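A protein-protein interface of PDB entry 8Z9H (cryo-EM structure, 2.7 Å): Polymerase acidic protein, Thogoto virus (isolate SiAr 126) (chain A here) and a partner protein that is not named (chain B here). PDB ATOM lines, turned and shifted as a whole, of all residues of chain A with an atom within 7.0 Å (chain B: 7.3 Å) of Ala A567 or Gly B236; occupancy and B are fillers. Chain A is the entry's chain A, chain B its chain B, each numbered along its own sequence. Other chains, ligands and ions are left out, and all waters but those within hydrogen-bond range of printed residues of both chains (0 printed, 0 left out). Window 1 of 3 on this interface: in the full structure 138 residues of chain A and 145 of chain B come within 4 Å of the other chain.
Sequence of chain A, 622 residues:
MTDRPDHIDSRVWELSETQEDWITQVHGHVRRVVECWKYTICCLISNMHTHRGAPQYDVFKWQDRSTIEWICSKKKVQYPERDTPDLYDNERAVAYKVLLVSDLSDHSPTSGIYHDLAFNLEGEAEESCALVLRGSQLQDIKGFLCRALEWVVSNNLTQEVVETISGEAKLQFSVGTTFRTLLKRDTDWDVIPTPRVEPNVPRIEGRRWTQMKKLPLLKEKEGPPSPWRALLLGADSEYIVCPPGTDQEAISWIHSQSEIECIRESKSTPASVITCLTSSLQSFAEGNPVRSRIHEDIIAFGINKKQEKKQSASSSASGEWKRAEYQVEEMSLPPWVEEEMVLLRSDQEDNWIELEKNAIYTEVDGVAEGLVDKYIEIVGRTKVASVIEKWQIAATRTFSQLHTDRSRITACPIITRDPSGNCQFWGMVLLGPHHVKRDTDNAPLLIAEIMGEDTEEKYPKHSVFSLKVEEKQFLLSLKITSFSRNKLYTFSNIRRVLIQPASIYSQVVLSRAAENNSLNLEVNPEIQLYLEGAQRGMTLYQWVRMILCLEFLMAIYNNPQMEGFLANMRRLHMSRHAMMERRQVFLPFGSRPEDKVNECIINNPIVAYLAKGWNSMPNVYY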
ATOM      1  N   PRO A 560      -0.356  21.100  25.633  1.00  0.00           N
ATOM      2  CA  PRO A 560      -1.436  22.101  25.689  1.00  0.00           C
ATOM      3  C   PRO A 560      -1.041  23.468  25.158  1.00  0.00           C
ATOM      4  O   PRO A 560      -1.859  24.127  24.503  1.00  0.00           O
ATOM      5  CB  PRO A 560      -1.776  22.162  27.185  1.00  0.00           C
ATOM      6  CG  PRO A 560      -1.234  20.903  27.785  1.00  0.00           C
ATOM      7  CD  PRO A 560      -0.435  20.160  26.762  1.00  0.00           C
ATOM      8  N   GLN A 561       0.190  23.915  25.418  1.00  0.00           N
ATOM      9  CA  GLN A 561       0.633  25.197  24.883  1.00  0.00           C
ATOM     10  C   GLN A 561       0.616  25.189  23.362  1.00  0.00           C
ATOM     11  O   GLN A 561       0.128  26.132  22.729  1.00  0.00           O
ATOM     12  CB  GLN A 561       2.032  25.532  25.400  1.00  0.00           C
ATOM     13  CG  GLN A 561       2.258  25.187  26.857  1.00  0.00           C
ATOM     14  CD  GLN A 561       3.663  25.514  27.312  1.00  0.00           C
ATOM     15  OE1 GLN A 561       4.344  26.343  26.711  1.00  0.00           O
ATOM     16  NE2 GLN A 561       4.109  24.858  28.376  1.00  0.00           N
ATOM     17  N   MET A 562       1.137  24.121  22.755  1.00  0.00           N
ATOM     18  CA  MET A 562       1.150  24.031  21.299  1.00  0.00           C
ATOM     19  C   MET A 562      -0.263  23.941  20.737  1.00  0.00           C
ATOM     20  O   MET A 562      -0.573  24.578  19.723  1.00  0.00           O
ATOM     21  CB  MET A 562       1.985  22.831  20.855  1.00  0.00           C
ATOM     22  CG  MET A 562       1.835  22.477  19.387  1.00  0.00           C
ATOM     23  SD  MET A 562       2.879  23.504  18.338  1.00  0.00           S
ATOM     24  CE  MET A 562       4.458  22.686  18.531  1.00  0.00           C
ATOM     25  N   GLU A 563      -1.133  23.159  21.382  1.00  0.00           N
ATOM     26  CA  GLU A 563      -2.511  23.043  20.917  1.00  0.00           C
ATOM     27  C   GLU A 563      -3.214  24.394  20.942  1.00  0.00           C
ATOM     28  O   GLU A 563      -3.849  24.793  19.961  1.00  0.00           O
ATOM     29  CB  GLU A 563      -3.272  22.028  21.769  1.00  0.00           C
ATOM     30  CG  GLU A 563      -2.680  20.633  21.762  1.00  0.00           C
ATOM     31  CD  GLU A 563      -3.286  19.751  20.690  1.00  0.00           C
ATOM     32  OE1 GLU A 563      -4.103  20.256  19.894  1.00  0.00           O
ATOM     33  OE2 GLU A 563      -2.946  18.551  20.644  1.00  0.00           O
ATOM     34  N   GLY A 564      -3.095  25.120  22.057  1.00  0.00           N
ATOM     35  CA  GLY A 564      -3.725  26.427  22.143  1.00  0.00           C
ATOM     36  C   GLY A 564      -3.142  27.423  21.160  1.00  0.00           C
ATOM     37  O   GLY A 564      -3.877  28.184  20.523  1.00  0.00           O
ATOM     38  N   PHE A 565      -1.814  27.428  21.018  1.00  0.00           N
ATOM     39  CA  PHE A 565      -1.162  28.347  20.093  1.00  0.00           C
ATOM     40  C   PHE A 565      -1.622  28.100  18.663  1.00  0.00           C
ATOM     41  O   PHE A 565      -1.962  29.040  17.937  1.00  0.00           O
ATOM     42  CB  PHE A 565       0.357  28.201  20.213  1.00  0.00           C
ATOM     43  CG  PHE A 565       1.131  28.976  19.185  1.00  0.00           C
ATOM     44  CD1 PHE A 565       1.468  30.299  19.407  1.00  0.00           C
ATOM     45  CD2 PHE A 565       1.538  28.376  18.006  1.00  0.00           C
ATOM     46  CE1 PHE A 565       2.184  31.013  18.469  1.00  0.00           C
ATOM     47  CE2 PHE A 565       2.252  29.086  17.065  1.00  0.00           C
ATOM     48  CZ  PHE A 565       2.575  30.405  17.296  1.00  0.00           C
ATOM     49  N   LEU A 566      -1.652  26.834  18.242  1.00  0.00           N
ATOM     50  CA  LEU A 566      -2.057  26.525  16.876  1.00  0.00           C
ATOM     51  C   LEU A 566      -3.542  26.785  16.665  1.00  0.00           C
ATOM     52  O   LEU A 566      -3.951  27.225  15.584  1.00  0.00           O
ATOM     53  CB  LEU A 566      -1.705  25.076  16.543  1.00  0.00           C
ATOM     54  CG  LEU A 566      -0.228  24.825  16.236  1.00  0.00           C
ATOM     55  CD1 LEU A 566      -0.039  23.460  15.611  1.00  0.00           C
ATOM     56  CD2 LEU A 566       0.323  25.907  15.323  1.00  0.00           C
ATOM     57  N   ALA A 567      -4.367  26.526  17.683  1.00  0.00           N
ATOM     58  CA  ALA A 567      -5.796  26.785  17.553  1.00  0.00           C
ATOM     59  C   ALA A 567      -6.081  28.275  17.419  1.00  0.00           C
ATOM     60  O   ALA A 567      -6.967  28.675  16.656  1.00  0.00           O
ATOM     61  CB  ALA A 567      -6.543  26.201  18.750  1.00  0.00           C
ATOM     62  N   ASN A 568      -5.352  29.111  18.156  1.00  0.00           N
ATOM     63  CA  ASN A 568      -5.603  30.545  18.126  1.00  0.00           C
ATOM     64  C   ASN A 568      -4.830  31.274  17.034  1.00  0.00           C
ATOM     65  O   ASN A 568      -5.144  32.434  16.748  1.00  0.00           O
ATOM     66  CB  ASN A 568      -5.276  31.160  19.487  1.00  0.00           C
ATOM     67  CG  ASN A 568      -6.260  30.745  20.559  1.00  0.00           C
ATOM     68  OD1 ASN A 568      -7.406  31.189  20.571  1.00  0.00           O
ATOM     69  ND2 ASN A 568      -5.817  29.882  21.465  1.00  0.00           N
ATOM     70  N   MET A 569      -3.837  30.632  16.415  1.00  0.00           N
ATOM     71  CA  MET A 569      -3.104  31.263  15.324  1.00  0.00           C
ATOM     72  C   MET A 569      -3.873  31.256  14.012  1.00  0.00           C
ATOM     73  O   MET A 569      -3.498  31.987  13.091  1.00  0.00           O
ATOM     74  CB  MET A 569      -1.757  30.564  15.124  1.00  0.00           C
ATOM     75  CG  MET A 569      -0.598  31.204  15.869  1.00  0.00           C
ATOM     76  SD  MET A 569      -0.705  33.000  15.944  1.00  0.00           S
ATOM     77  CE  MET A 569      -0.410  33.424  14.230  1.00  0.00           C
ATOM     78  N   ARG A 570      -4.924  30.442  13.902  1.00  0.00           N
ATOM     79  CA  ARG A 570      -5.662  30.351  12.647  1.00  0.00           C
ATOM     80  C   ARG A 570      -6.406  31.646  12.340  1.00  0.00           C
ATOM     81  O   ARG A 570      -6.496  32.052  11.177  1.00  0.00           O
ATOM     82  CB  ARG A 570      -6.616  29.162  12.694  1.00  0.00           C
ATOM     83  CG  ARG A 570      -5.899  27.846  12.940  1.00  0.00           C
ATOM     84  CD  ARG A 570      -6.836  26.754  13.409  1.00  0.00           C
ATOM     85  NE  ARG A 570      -6.094  25.615  13.931  1.00  0.00           N
ATOM     86  CZ  ARG A 570      -6.628  24.634  14.645  1.00  0.00           C
ATOM     87  NH1 ARG A 570      -7.916  24.619  14.941  1.00  0.00           N
ATOM     88  NH2 ARG A 570      -5.849  23.647  15.077  1.00  0.00           N
ATOM     89  N   ARG A 571      -6.939  32.310  13.368  1.00  0.00           N
ATOM     90  CA  ARG A 571      -7.593  33.596  13.149  1.00  0.00           C
ATOM     91  C   ARG A 571      -6.612  34.635  12.623  1.00  0.00           C
ATOM     92  O   ARG A 571      -6.930  35.387  11.696  1.00  0.00           O
ATOM     93  CB  ARG A 571      -8.244  34.084  14.442  1.00  0.00           C
ATOM     94  CG  ARG A 571      -9.469  33.295  14.853  1.00  0.00           C
ATOM     95  CD  ARG A 571     -10.139  33.916  16.062  1.00  0.00           C
ATOM     96  NE  ARG A 571      -9.290  33.844  17.244  1.00  0.00           N
ATOM     97  CZ  ARG A 571      -9.240  32.802  18.062  1.00  0.00           C
ATOM     98  NH1 ARG A 571      -9.979  31.725  17.855  1.00  0.00           N
ATOM     99  NH2 ARG A 571      -8.426  32.841  19.112  1.00  0.00           N
ATOM    100  N   VAL A 597      -3.199  34.119  21.847  1.00  0.00           N
ATOM    101  CA  VAL A 597      -2.008  33.427  21.370  1.00  0.00           C
ATOM    102  C   VAL A 597      -0.855  33.583  22.352  1.00  0.00           C
ATOM    103  O   VAL A 597      -0.104  32.635  22.595  1.00  0.00           O
ATOM    104  CB  VAL A 597      -1.628  33.947  19.970  1.00  0.00           C
ATOM    105  CG1 VAL A 597      -0.342  33.303  19.496  1.00  0.00           C
ATOM    106  CG2 VAL A 597      -2.752  33.690  18.984  1.00  0.00           C
ATOM    107  N   GLN B  16      -3.989  26.368   6.048  1.00  0.00           N
ATOM    108  CA  GLN B  16      -4.605  26.231   7.363  1.00  0.00           C
ATOM    109  C   GLN B  16      -4.484  24.813   7.901  1.00  0.00           C
ATOM    110  O   GLN B  16      -4.495  24.619   9.121  1.00  0.00           O
ATOM    111  CB  GLN B  16      -6.080  26.632   7.310  1.00  0.00           C
ATOM    112  CG  GLN B  16      -6.330  28.114   7.100  1.00  0.00           C
ATOM    113  CD  GLN B  16      -5.916  28.946   8.293  1.00  0.00           C
ATOM    114  OE1 GLN B  16      -5.419  30.059   8.144  1.00  0.00           O
ATOM    115  NE2 GLN B  16      -6.114  28.405   9.486  1.00  0.00           N
ATOM    116  N   LEU B  19      -1.558  24.244  10.290  1.00  0.00           N
ATOM    117  CA  LEU B  19      -1.664  24.724  11.666  1.00  0.00           C
ATOM    118  C   LEU B  19      -2.394  23.713  12.541  1.00  0.00           C
ATOM    119  O   LEU B  19      -3.333  24.039  13.264  1.00  0.00           O
ATOM    120  CB  LEU B  19      -2.363  26.078  11.693  1.00  0.00           C
ATOM    121  CG  LEU B  19      -1.773  27.152  10.780  1.00  0.00           C
ATOM    122  CD1 LEU B  19      -2.534  28.457  10.930  1.00  0.00           C
ATOM    123  CD2 LEU B  19      -0.300  27.348  11.075  1.00  0.00           C
ATOM    124  N   TYR B  20      -1.944  22.463  12.479  1.00  0.00           N
ATOM    125  CA  TYR B  20      -2.560  21.366  13.219  1.00  0.00           C
ATOM    126  C   TYR B  20      -1.444  20.450  13.696  1.00  0.00           C
ATOM    127  O   TYR B  20      -0.758  19.830  12.879  1.00  0.00           O
ATOM    128  CB  TYR B  20      -3.560  20.599  12.353  1.00  0.00           C
ATOM    129  CG  TYR B  20      -4.915  21.256  12.241  1.00  0.00           C
ATOM    130  CD1 TYR B  20      -5.143  22.273  11.325  1.00  0.00           C
ATOM    131  CD2 TYR B  20      -5.969  20.860  13.052  1.00  0.00           C
ATOM    132  CE1 TYR B  20      -6.378  22.875  11.219  1.00  0.00           C
ATOM    133  CE2 TYR B  20      -7.209  21.457  12.954  1.00  0.00           C
ATOM    134  CZ  TYR B  20      -7.407  22.464  12.036  1.00  0.00           C
ATOM    135  OH  TYR B  20      -8.641  23.063  11.934  1.00  0.00           O
ATOM    136  N   TYR B  22      -1.803  17.676  15.137  1.00  0.00           N
ATOM    137  CA  TYR B  22      -2.327  16.335  15.321  1.00  0.00           C
ATOM    138  C   TYR B  22      -1.298  15.312  14.842  1.00  0.00           C
ATOM    139  O   TYR B  22      -0.276  15.654  14.239  1.00  0.00           O
ATOM    140  CB  TYR B  22      -3.660  16.164  14.590  1.00  0.00           C
ATOM    141  CG  TYR B  22      -4.786  17.057  15.091  1.00  0.00           C
ATOM    142  CD1 TYR B  22      -4.575  17.997  16.092  1.00  0.00           C
ATOM    143  CD2 TYR B  22      -6.065  16.947  14.568  1.00  0.00           C
ATOM    144  CE1 TYR B  22      -5.597  18.808  16.541  1.00  0.00           C
ATOM    145  CE2 TYR B  22      -7.094  17.751  15.013  1.00  0.00           C
ATOM    146  CZ  TYR B  22      -6.854  18.679  15.999  1.00  0.00           C
ATOM    147  OH  TYR B  22      -7.878  19.481  16.447  1.00  0.00           O
ATOM    148  N   PRO B  27      -3.529  16.648  24.927  1.00  0.00           N
ATOM    149  CA  PRO B  27      -3.414  16.930  26.361  1.00  0.00           C
ATOM    150  C   PRO B  27      -4.472  16.200  27.172  1.00  0.00           C
ATOM    151  O   PRO B  27      -5.587  15.950  26.708  1.00  0.00           O
ATOM    152  CB  PRO B  27      -3.603  18.449  26.441  1.00  0.00           C
ATOM    153  CG  PRO B  27      -4.364  18.799  25.215  1.00  0.00           C
ATOM    154  CD  PRO B  27      -3.901  17.844  24.155  1.00  0.00           C
ATOM    155  N   GLU B 234      -8.752  16.120  24.709  1.00  0.00           N
ATOM    156  CA  GLU B 234      -9.352  17.214  23.959  1.00  0.00           C
ATOM    157  C   GLU B 234      -8.250  18.100  23.397  1.00  0.00           C
ATOM    158  O   GLU B 234      -7.309  18.458  24.113  1.00  0.00           O
ATOM    159  CB  GLU B 234     -10.293  18.039  24.838  1.00  0.00           C
ATOM    160  CG  GLU B 234     -10.716  19.352  24.202  1.00  0.00           C
ATOM    161  CD  GLU B 234     -11.834  20.037  24.956  1.00  0.00           C
ATOM    162  OE1 GLU B 234     -12.810  19.358  25.326  1.00  0.00           O
ATOM    163  OE2 GLU B 234     -11.733  21.259  25.181  1.00  0.00           O
ATOM    164  N   ARG B 235      -8.369  18.454  22.122  1.00  0.00           N
ATOM    165  CA  ARG B 235      -7.353  19.220  21.422  1.00  0.00           C
ATOM    166  C   ARG B 235      -7.858  20.625  21.122  1.00  0.00           C
ATOM    167  O   ARG B 235      -9.063  20.856  20.989  1.00  0.00           O
ATOM    168  CB  ARG B 235      -6.952  18.523  20.119  1.00  0.00           C
ATOM    169  CG  ARG B 235      -6.912  17.008  20.223  1.00  0.00           C
ATOM    170  CD  ARG B 235      -6.369  16.378  18.956  1.00  0.00           C
ATOM    171  NE  ARG B 235      -4.913  16.402  18.919  1.00  0.00           N
ATOM    172  CZ  ARG B 235      -4.145  15.321  18.931  1.00  0.00           C
ATOM    173  NH1 ARG B 235      -4.663  14.106  18.960  1.00  0.00           N
ATOM    174  NH2 ARG B 235      -2.824  15.465  18.907  1.00  0.00           N
ATOM    175  N   GLY B 236      -6.922  21.563  21.022  1.00  0.00           N
ATOM    176  CA  GLY B 236      -7.234  22.921  20.635  1.00  0.00           C
ATOM    177  C   GLY B 236      -7.442  23.909  21.761  1.00  0.00           C
ATOM    178  O   GLY B 236      -7.900  25.025  21.498  1.00  0.00           O
ATOM    179  N   ARG B 237      -7.124  23.543  23.000  1.00  0.00           N
ATOM    180  CA  ARG B 237      -7.296  24.441  24.131  1.00  0.00           C
ATOM    181  C   ARG B 237      -6.119  24.306  25.084  1.00  0.00           C
ATOM    182  O   ARG B 237      -5.610  23.205  25.306  1.00  0.00           O
ATOM    183  CB  ARG B 237      -8.606  24.167  24.876  1.00  0.00           C
ATOM    184  CG  ARG B 237      -9.834  24.741  24.194  1.00  0.00           C
ATOM    185  CD  ARG B 237     -11.105  24.324  24.906  1.00  0.00           C
ATOM    186  NE  ARG B 237     -10.912  24.230  26.348  1.00  0.00           N
ATOM    187  CZ  ARG B 237     -11.204  25.197  27.207  1.00  0.00           C
ATOM    188  NH1 ARG B 237     -11.715  26.348  26.803  1.00  0.00           N
ATOM    189  NH2 ARG B 237     -10.976  25.004  28.503  1.00  0.00           N
ATOM    190  N   LEU B 238      -5.691  25.440  25.641  1.00  0.00           N
ATOM    191  CA  LEU B 238      -4.589  25.434  26.598  1.00  0.00           C
ATOM    192  C   LEU B 238      -5.029  24.894  27.954  1.00  0.00           C
ATOM    193  O   LEU B 238      -4.295  24.129  28.591  1.00  0.00           O
ATOM    194  CB  LEU B 238      -4.018  26.844  26.740  1.00  0.00           C
ATOM    195  CG  LEU B 238      -2.977  27.081  27.834  1.00  0.00           C
ATOM    196  CD1 LEU B 238      -1.666  26.404  27.489  1.00  0.00           C
ATOM    197  CD2 LEU B 238      -2.771  28.567  28.060  1.00  0.00           C
ATOM    198  N   ASN B 239      -6.218  25.276  28.409  1.00  0.00           N
ATOM    199  CA  ASN B 239      -6.697  24.937  29.742  1.00  0.00           C
ATOM    200  C   ASN B 239      -7.726  23.817  29.675  1.00  0.00           C
ATOM    201  O   ASN B 239      -8.627  23.836  28.833  1.00  0.00           O
ATOM    202  CB  ASN B 239      -7.309  26.162  30.424  1.00  0.00           C
ATOM    203  CG  ASN B 239      -6.338  27.319  30.522  1.00  0.00           C
ATOM    204  OD1 ASN B 239      -6.667  28.451  30.169  1.00  0.00           O
ATOM    205  ND2 ASN B 239      -5.133  27.040  31.002  1.00  0.00           N
ATOM    206  N   ARG B 240      -7.584  22.843  30.571  1.00  0.00           N
ATOM    207  CA  ARG B 240      -8.527  21.736  30.635  1.00  0.00           C
ATOM    208  C   ARG B 240      -9.893  22.225  31.099  1.00  0.00           C
ATOM    209  O   ARG B 240      -9.999  23.080  31.982  1.00  0.00           O
ATOM    210  CB  ARG B 240      -8.013  20.651  31.581  1.00  0.00           C
ATOM    211  CG  ARG B 240      -6.563  20.238  31.363  1.00  0.00           C
ATOM    212  CD  ARG B 240      -6.398  19.282  30.184  1.00  0.00           C
ATOM    213  NE  ARG B 240      -6.504  19.961  28.898  1.00  0.00           N
ATOM    214  CZ  ARG B 240      -5.582  20.774  28.399  1.00  0.00           C
ATOM    215  NH1 ARG B 240      -4.451  21.014  29.042  1.00  0.00           N
ATOM    216  NH2 ARG B 240      -5.800  21.360  27.225  1.00  0.00           N
ATOM    217  N   LYS B 458     -12.089  36.773  19.428  1.00  0.00           N
ATOM    218  CA  LYS B 458     -12.346  35.692  18.488  1.00  0.00           C
ATOM    219  C   LYS B 458     -13.299  36.080  17.366  1.00  0.00           C
ATOM    220  O   LYS B 458     -13.659  35.219  16.557  1.00  0.00           O
ATOM    221  CB  LYS B 458     -12.898  34.471  19.230  1.00  0.00           C
ATOM    222  CG  LYS B 458     -11.922  33.851  20.213  1.00  0.00           C
ATOM    223  CD  LYS B 458     -12.469  32.556  20.784  1.00  0.00           C
ATOM    224  CE  LYS B 458     -11.429  31.843  21.628  1.00  0.00           C
ATOM    225  NZ  LYS B 458     -11.896  30.502  22.072  1.00  0.00           N
ATOM    226  N   PHE B 474     -12.716  26.656   6.701  1.00  0.00           N
ATOM    227  CA  PHE B 474     -12.252  27.910   6.129  1.00  0.00           C
ATOM    228  C   PHE B 474     -12.629  27.979   4.656  1.00  0.00           C
ATOM    229  O   PHE B 474     -12.528  26.985   3.933  1.00  0.00           O
ATOM    230  CB  PHE B 474     -10.737  28.054   6.287  1.00  0.00           C
ATOM    231  CG  PHE B 474     -10.296  28.311   7.698  1.00  0.00           C
ATOM    232  CD1 PHE B 474     -10.050  27.260   8.563  1.00  0.00           C
ATOM    233  CD2 PHE B 474     -10.123  29.606   8.158  1.00  0.00           C
ATOM    234  CE1 PHE B 474      -9.642  27.495   9.860  1.00  0.00           C
ATOM    235  CE2 PHE B 474      -9.713  29.846   9.454  1.00  0.00           C
ATOM    236  CZ  PHE B 474      -9.474  28.789  10.306  1.00  0.00           C
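NE of Arg B235 is in salt-bridge range of OE2 of Glu A563, at 3.4 Å. The side-chain carboxylate of Glu A563 lies within hydrogen-bond range of the backbone NH of Gly B236. The guanidinium group (NH2) of Arg A570 sits at hydrogen-bond distance from the backbone carbonyl oxygen (O) of Leu B19 (3.1 Å). OH of Tyr B20 is in hydrogen-bond range of NH1 of Arg A570 (3.5 Å).
The guanidinium group (NE) of Arg A570 lies within hydrogen-bond range of the backbone carbonyl oxygen (O) of Leu A566, 3.1 Å away. The guanidinium group (NH2) of Arg A571 sits at hydrogen-bond distance from the side-chain amide oxygen (OD1) of Asn A568. The guanidinium group (NE) of Arg B237 is in salt-bridge range of the side-chain carboxylate (OE2) of Glu B234 (3.3 Å). The backbone carbonyl oxygen of Asn B239 lies within hydrogen-bond range of the guanidinium group of Arg B237. The backbone carbonyl oxygen of Arg B237 sits at hydrogen-bond distance from the guanidinium group of Arg B240. NH1 of Arg B240 sits at hydrogen-bond distance from O of Leu B238 (3.2 Å).
Arg B237 touches Pro A560 (O to O, 3.9 Å). CB of Pro A560 touches O of Leu B238, at 3.5 Å. Leu B238 touches Gln A561. Tyr B22 touches Glu A563. Glu A563 touches Pro B27 (OE2 to CD, 3.7 Å). Leu B19 touches Leu A566 (O to CB, 3.8 Å). CD1 of Leu A566 touches N of Tyr B20 (3.8 Å). O of Gly B236 touches CB of Ala A567, at 3.3 Å. Arg A570 touches Phe B474 (CB to CZ, 3.7 Å). CG of Lys B458 touches CZ of Arg A571 (3.6 Å).
Printed residues of chain B within 4 Å of Gln A561: Leu B238 (3.7 Å). Gly A564 touches none of the printed residues of chain B. Of the printed residues of chain B, Leu A566 touches Leu B19 and Tyr B20. Ala A567 touches just one residue of chain B: Gly B236 (3.3 Å). Of the printed residues of chain B, Arg A570 touches Gln B16, Leu B19, Tyr B20 and Phe B474. Printed residues of chain B within 4 Å of Arg A571: Lys B458. Glu B234 touches none of the printed residues of chain A. Gly B236 touches just these residues of chain A: Glu A563 and Ala A567. Of the printed residues of chain A, Arg B237 touches Pro A560. The nearest residue of chain A that does not touch Gly B236 is Gly A564 (4.5 Å). The nearest printed residue of chain A that does not touch Arg B235 is Ala A567 (6.2 Å).
Of the 14 printed residues of chain B, 12 touch a printed residue of chain A. Hydrophobic or aromatic side chains of chain B within 4 Å of the printed part of chain A: Leu B19, Tyr B20, Tyr B22, Pro B27, Leu B238 and Phe B474. Of the 13 printed residues of chain A, 7 touch a printed residue of chain B.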
